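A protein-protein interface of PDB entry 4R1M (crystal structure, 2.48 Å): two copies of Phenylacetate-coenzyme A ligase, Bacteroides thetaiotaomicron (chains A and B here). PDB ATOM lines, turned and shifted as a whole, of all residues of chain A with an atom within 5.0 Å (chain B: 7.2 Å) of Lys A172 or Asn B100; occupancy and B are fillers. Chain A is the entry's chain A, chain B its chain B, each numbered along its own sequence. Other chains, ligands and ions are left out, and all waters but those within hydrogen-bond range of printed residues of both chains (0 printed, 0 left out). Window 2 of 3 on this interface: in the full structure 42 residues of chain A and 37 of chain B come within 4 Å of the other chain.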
ATOM      1  N   LYS A 168       6.628  14.919   2.396  1.00  0.00           N
ATOM      2  CA  LYS A 168       6.938  15.498   3.706  1.00  0.00           C
ATOM      3  C   LYS A 168       7.801  14.536   4.538  1.00  0.00           C
ATOM      4  O   LYS A 168       8.731  14.977   5.203  1.00  0.00           O
ATOM      5  CB  LYS A 168       5.677  15.894   4.498  1.00  0.00           C
ATOM      6  CG  LYS A 168       5.074  17.229   4.088  1.00  0.00           C
ATOM      7  CD  LYS A 168       3.953  17.647   5.014  1.00  0.00           C
ATOM      8  N   ARG A 169       7.534  13.227   4.458  1.00  0.00           N
ATOM      9  CA  ARG A 169       8.321  12.216   5.184  1.00  0.00           C
ATOM     10  C   ARG A 169       9.733  12.063   4.519  1.00  0.00           C
ATOM     11  O   ARG A 169      10.714  11.838   5.228  1.00  0.00           O
ATOM     12  CB  ARG A 169       7.567  10.889   5.232  1.00  0.00           C
ATOM     13  CG  ARG A 169       7.978   9.949   6.351  1.00  0.00           C
ATOM     14  CD  ARG A 169       7.320   8.595   6.198  1.00  0.00           C
ATOM     15  NE  ARG A 169       7.986   7.809   5.161  1.00  0.00           N
ATOM     16  CZ  ARG A 169       7.754   6.524   4.910  1.00  0.00           C
ATOM     17  NH1 ARG A 169       6.866   5.847   5.631  1.00  0.00           N
ATOM     18  NH2 ARG A 169       8.409   5.903   3.937  1.00  0.00           N
ATOM     19  N   GLN A 170       9.835  12.270   3.183  1.00  0.00           N
ATOM     20  CA  GLN A 170      11.119  12.196   2.454  1.00  0.00           C
ATOM     21  C   GLN A 170      12.089  13.293   2.938  1.00  0.00           C
ATOM     22  O   GLN A 170      13.276  13.039   3.125  1.00  0.00           O
ATOM     23  CB  GLN A 170      10.916  12.325   0.922  1.00  0.00           C
ATOM     24  CG  GLN A 170      10.003  11.279   0.258  1.00  0.00           C
ATOM     25  CD  GLN A 170      10.640   9.936  -0.029  1.00  0.00           C
ATOM     26  OE1 GLN A 170      11.859   9.756   0.042  1.00  0.00           O
ATOM     27  NE2 GLN A 170       9.824   8.988  -0.485  1.00  0.00           N
ATOM     28  N   ILE A 171      11.562  14.500   3.138  1.00  0.00           N
ATOM     29  CA  ILE A 171      12.265  15.699   3.591  1.00  0.00           C
ATOM     30  C   ILE A 171      12.625  15.529   5.084  1.00  0.00           C
ATOM     31  O   ILE A 171      13.702  15.937   5.493  1.00  0.00           O
ATOM     32  CB  ILE A 171      11.347  16.934   3.299  1.00  0.00           C
ATOM     33  CG1 ILE A 171      11.596  17.467   1.881  1.00  0.00           C
ATOM     34  CG2 ILE A 171      11.547  18.112   4.289  1.00  0.00           C
ATOM     35  CD1 ILE A 171      11.399  16.628   0.790  1.00  0.00           C
ATOM     36  N   LYS A 172      11.748  14.893   5.866  1.00  0.00           N
ATOM     37  CA  LYS A 172      11.990  14.616   7.276  1.00  0.00           C
ATOM     38  C   LYS A 172      13.193  13.660   7.410  1.00  0.00           C
ATOM     39  O   LYS A 172      14.085  13.935   8.218  1.00  0.00           O
ATOM     40  CB  LYS A 172      10.726  14.041   7.951  1.00  0.00           C
ATOM     41  CG  LYS A 172      10.901  13.770   9.438  1.00  0.00           C
ATOM     42  CD  LYS A 172       9.692  13.136  10.102  1.00  0.00           C
ATOM     43  CE  LYS A 172       9.946  12.785  11.543  1.00  0.00           C
ATOM     44  NZ  LYS A 172      10.270  13.987  12.343  1.00  0.00           N
ATOM     45  N   PHE A 173      13.235  12.580   6.599  1.00  0.00           N
ATOM     46  CA  PHE A 173      14.337  11.618   6.597  1.00  0.00           C
ATOM     47  C   PHE A 173      15.662  12.307   6.241  1.00  0.00           C
ATOM     48  O   PHE A 173      16.650  12.100   6.947  1.00  0.00           O
ATOM     49  CB  PHE A 173      14.065  10.451   5.626  1.00  0.00           C
ATOM     50  CG  PHE A 173      12.954   9.482   6.002  1.00  0.00           C
ATOM     51  CD1 PHE A 173      12.401   9.479   7.284  1.00  0.00           C
ATOM     52  CD2 PHE A 173      12.512   8.523   5.100  1.00  0.00           C
ATOM     53  CE1 PHE A 173      11.392   8.569   7.630  1.00  0.00           C
ATOM     54  CE2 PHE A 173      11.520   7.592   5.462  1.00  0.00           C
ATOM     55  CZ  PHE A 173      10.962   7.627   6.720  1.00  0.00           C
ATOM     56  N   ILE A 174      15.668  13.170   5.199  1.00  0.00           N
ATOM     57  CA  ILE A 174      16.865  13.889   4.754  1.00  0.00           C
ATOM     58  C   ILE A 174      17.370  14.798   5.881  1.00  0.00           C
ATOM     59  O   ILE A 174      18.562  14.801   6.162  1.00  0.00           O
ATOM     60  CB  ILE A 174      16.594  14.695   3.439  1.00  0.00           C
ATOM     61  CG1 ILE A 174      16.352  13.704   2.248  1.00  0.00           C
ATOM     62  CG2 ILE A 174      17.746  15.708   3.129  1.00  0.00           C
ATOM     63  CD1 ILE A 174      15.661  14.306   1.056  1.00  0.00           C
ATOM     64  N   SER A 175      16.458  15.520   6.539  1.00  0.00           N
ATOM     65  CA  SER A 175      16.764  16.461   7.614  1.00  0.00           C
ATOM     66  C   SER A 175      17.249  15.744   8.886  1.00  0.00           C
ATOM     67  O   SER A 175      18.284  16.127   9.433  1.00  0.00           O
ATOM     68  CB  SER A 175      15.540  17.313   7.942  1.00  0.00           C
ATOM     69  OG  SER A 175      15.097  18.040   6.807  1.00  0.00           O
ATOM     70  N   ASP A 176      16.515  14.721   9.353  1.00  0.00           N
ATOM     71  CA  ASP A 176      16.801  14.007  10.593  1.00  0.00           C
ATOM     72  C   ASP A 176      17.905  12.943  10.452  1.00  0.00           C
ATOM     73  O   ASP A 176      18.615  12.718  11.426  1.00  0.00           O
ATOM     74  CB  ASP A 176      15.520  13.316  11.103  1.00  0.00           C
ATOM     75  CG  ASP A 176      14.328  14.229  11.424  1.00  0.00           C
ATOM     76  OD1 ASP A 176      14.504  15.477  11.430  1.00  0.00           O
ATOM     77  OD2 ASP A 176      13.235  13.696  11.695  1.00  0.00           O
ATOM     78  N   PHE A 177      18.032  12.258   9.289  1.00  0.00           N
ATOM     79  CA  PHE A 177      19.041  11.194   9.165  1.00  0.00           C
ATOM     80  C   PHE A 177      20.306  11.692   8.454  1.00  0.00           C
ATOM     81  O   PHE A 177      21.279  10.947   8.365  1.00  0.00           O
ATOM     82  CB  PHE A 177      18.478   9.953   8.426  1.00  0.00           C
ATOM     83  CG  PHE A 177      17.194   9.382   9.009  1.00  0.00           C
ATOM     84  CD1 PHE A 177      16.877   9.552  10.362  1.00  0.00           C
ATOM     85  CD2 PHE A 177      16.341   8.607   8.225  1.00  0.00           C
ATOM     86  CE1 PHE A 177      15.683   9.047  10.889  1.00  0.00           C
ATOM     87  CE2 PHE A 177      15.166   8.066   8.765  1.00  0.00           C
ATOM     88  CZ  PHE A 177      14.835   8.309  10.087  1.00  0.00           C
ATOM     89  N   LYS B  68       8.979   3.649  25.477  1.00  0.00           N
ATOM     90  CA  LYS B  68       8.724   4.264  24.190  1.00  0.00           C
ATOM     91  C   LYS B  68       8.943   5.775  24.321  1.00  0.00           C
ATOM     92  O   LYS B  68       9.540   6.382  23.424  1.00  0.00           O
ATOM     93  CB  LYS B  68       7.300   3.892  23.733  1.00  0.00           C
ATOM     94  CG  LYS B  68       6.800   4.514  22.421  1.00  0.00           C
ATOM     95  CD  LYS B  68       7.696   4.343  21.191  1.00  0.00           C
ATOM     96  CE  LYS B  68       7.988   2.929  20.781  1.00  0.00           C
ATOM     97  NZ  LYS B  68       9.457   2.705  20.791  1.00  0.00           N
ATOM     98  N   ARG B  72      11.364   8.200  22.284  1.00  0.00           N
ATOM     99  CA  ARG B  72      10.878   9.370  21.533  1.00  0.00           C
ATOM    100  C   ARG B  72      11.673  10.610  21.912  1.00  0.00           C
ATOM    101  O   ARG B  72      12.007  11.411  21.047  1.00  0.00           O
ATOM    102  CB  ARG B  72       9.385   9.613  21.773  1.00  0.00           C
ATOM    103  CG  ARG B  72       8.470   8.597  21.095  1.00  0.00           C
ATOM    104  CD  ARG B  72       7.033   8.882  21.495  1.00  0.00           C
ATOM    105  NE  ARG B  72       6.086   8.050  20.754  1.00  0.00           N
ATOM    106  CZ  ARG B  72       5.099   7.351  21.306  1.00  0.00           C
ATOM    107  NH1 ARG B  72       4.915   7.370  22.623  1.00  0.00           N
ATOM    108  NH2 ARG B  72       4.292   6.621  20.548  1.00  0.00           N
ATOM    109  N   TYR B  75      15.050  10.607  20.092  1.00  0.00           N
ATOM    110  CA  TYR B  75      14.950  10.528  18.640  1.00  0.00           C
ATOM    111  C   TYR B  75      15.893  11.548  17.944  1.00  0.00           C
ATOM    112  O   TYR B  75      15.915  12.722  18.316  1.00  0.00           O
ATOM    113  CB  TYR B  75      13.498  10.783  18.194  1.00  0.00           C
ATOM    114  CG  TYR B  75      13.330  10.917  16.694  1.00  0.00           C
ATOM    115  CD1 TYR B  75      13.143   9.796  15.891  1.00  0.00           C
ATOM    116  CD2 TYR B  75      13.362  12.167  16.075  1.00  0.00           C
ATOM    117  CE1 TYR B  75      13.026   9.913  14.501  1.00  0.00           C
ATOM    118  CE2 TYR B  75      13.242  12.297  14.687  1.00  0.00           C
ATOM    119  CZ  TYR B  75      13.064  11.165  13.905  1.00  0.00           C
ATOM    120  OH  TYR B  75      12.950  11.270  12.541  1.00  0.00           O
ATOM    121  N   PRO B  76      16.628  11.143  16.886  1.00  0.00           N
ATOM    122  CA  PRO B  76      16.649   9.803  16.262  1.00  0.00           C
ATOM    123  C   PRO B  76      17.772   8.855  16.713  1.00  0.00           C
ATOM    124  O   PRO B  76      17.571   7.649  16.593  1.00  0.00           O
ATOM    125  CB  PRO B  76      16.881  10.129  14.780  1.00  0.00           C
ATOM    126  CG  PRO B  76      17.535  11.511  14.744  1.00  0.00           C
ATOM    127  CD  PRO B  76      17.458  12.106  16.126  1.00  0.00           C
ATOM    128  N   SER B  93      11.974   2.055  10.374  1.00  0.00           N
ATOM    129  CA  SER B  93      10.985   2.877  11.075  1.00  0.00           C
ATOM    130  C   SER B  93       9.657   2.099  11.413  1.00  0.00           C
ATOM    131  O   SER B  93       9.390   1.023  10.852  1.00  0.00           O
ATOM    132  CB  SER B  93      10.657   4.090  10.222  1.00  0.00           C
ATOM    133  OG  SER B  93       9.748   4.930  10.907  1.00  0.00           O
ATOM    134  N   SER B  94       8.843   2.662  12.363  1.00  0.00           N
ATOM    135  CA  SER B  94       7.486   2.211  12.741  1.00  0.00           C
ATOM    136  C   SER B  94       6.604   3.430  13.085  1.00  0.00           C
ATOM    137  O   SER B  94       7.106   4.514  13.399  1.00  0.00           O
ATOM    138  CB  SER B  94       7.492   1.209  13.897  1.00  0.00           C
ATOM    139  OG  SER B  94       7.828   1.755  15.164  1.00  0.00           O
ATOM    140  N   GLY B  99       3.238  10.290  16.496  1.00  0.00           N
ATOM    141  CA  GLY B  99       4.029  11.517  16.478  1.00  0.00           C
ATOM    142  C   GLY B  99       5.332  11.366  15.712  1.00  0.00           C
ATOM    143  O   GLY B  99       5.327  11.377  14.470  1.00  0.00           O
ATOM    144  N   ASN B 100       6.468  11.254  16.454  1.00  0.00           N
ATOM    145  CA  ASN B 100       7.787  10.999  15.865  1.00  0.00           C
ATOM    146  C   ASN B 100       7.950   9.505  15.713  1.00  0.00           C
ATOM    147  O   ASN B 100       7.518   8.760  16.607  1.00  0.00           O
ATOM    148  CB  ASN B 100       8.936  11.610  16.661  1.00  0.00           C
ATOM    149  CG  ASN B 100       9.564  12.798  15.978  1.00  0.00           C
ATOM    150  OD1 ASN B 100       9.367  13.045  14.783  1.00  0.00           O
ATOM    151  ND2 ASN B 100      10.349  13.558  16.719  1.00  0.00           N
ATOM    152  N   PRO B 101       8.493   9.035  14.566  1.00  0.00           N
ATOM    153  CA  PRO B 101       8.624   7.585  14.363  1.00  0.00           C
ATOM    154  C   PRO B 101       9.729   6.988  15.227  1.00  0.00           C
ATOM    155  O   PRO B 101      10.551   7.734  15.804  1.00  0.00           O
ATOM    156  CB  PRO B 101       8.971   7.479  12.874  1.00  0.00           C
ATOM    157  CG  PRO B 101       9.752   8.720  12.597  1.00  0.00           C
ATOM    158  CD  PRO B 101       9.068   9.787  13.430  1.00  0.00           C
ATOM    159  N   THR B 102       9.759   5.657  15.326  1.00  0.00           N
ATOM    160  CA  THR B 102      10.858   5.074  16.077  1.00  0.00           C
ATOM    161  C   THR B 102      11.828   4.525  15.058  1.00  0.00           C
ATOM    162  O   THR B 102      11.434   3.835  14.108  1.00  0.00           O
ATOM    163  CB  THR B 102      10.432   4.060  17.126  1.00  0.00           C
ATOM    164  OG1 THR B 102       9.852   2.893  16.525  1.00  0.00           O
ATOM    165  CG2 THR B 102       9.549   4.686  18.169  1.00  0.00           C
ATOM    166  N   VAL B 103      13.100   4.857  15.281  1.00  0.00           N
ATOM    167  CA  VAL B 103      14.224   4.529  14.440  1.00  0.00           C
ATOM    168  C   VAL B 103      15.074   3.458  15.122  1.00  0.00           C
ATOM    169  O   VAL B 103      15.411   3.582  16.286  1.00  0.00           O
ATOM    170  CB  VAL B 103      15.026   5.840  14.168  1.00  0.00           C
ATOM    171  CG1 VAL B 103      16.377   5.583  13.525  1.00  0.00           C
ATOM    172  CG2 VAL B 103      14.218   6.811  13.342  1.00  0.00           C
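CE of Lys A172 touches OH of Tyr B75 (3.5 Å). Pro B101 touches Lys A172. Pro B76 touches Asp A176. Tyr B75 touches Phe A177 (OH to CE1, 3.9 Å). Phe A177 touches Val B103 (CE1 to CG2, 3.6 Å).
No position is printed for both chains.
Of the 10 printed residues of chain A, 3 touch a printed residue of chain B. Hydrophobic or aromatic side chains of chain A within 4 Å of the printed part of chain B: Phe A177.
The side-chain amino group (NZ) of Lys A172 sits at hydrogen-bond distance from the side-chain amide oxygen (OD1) of Asn B100 (2.8 Å). The side-chain carboxylate (OD2) of Asp A176 lies within hydrogen-bond range of the side-chain hydroxyl (OH) of Tyr B75 (2.6 Å).
Lys A172 touches just these residues of chain B: Tyr B75, Asn B100 and Pro B101. Of chain A, only Lys A172 (2.8 Å) comes within 4 Å of Asn B100. Printed residues of chain B within 4 Å of Asp A176: Tyr B75 (2.6 Å) and Pro B76 (3.7 Å). Printed residues of chain A within 4 Å of Pro B101: Lys A172. Printed residues of chain A within 4 Å of Val B103: Phe A177 (3.6 Å). Phe A173 touches none of the printed residues of chain B. Arg B72 touches none of the printed residues of chain A. The nearest residue of chain B that does not touch Lys A172 is Gly B99 (5.6 Å). The nearest printed residue of chain A that does not touch Asn B100 is Asp A176 (5.0 Å).
The side-chain amino group (NZ) of Lys A172 lies within salt-bridge range of the side-chain carboxylate (OD2) of Asp A176 (3.0 Å).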
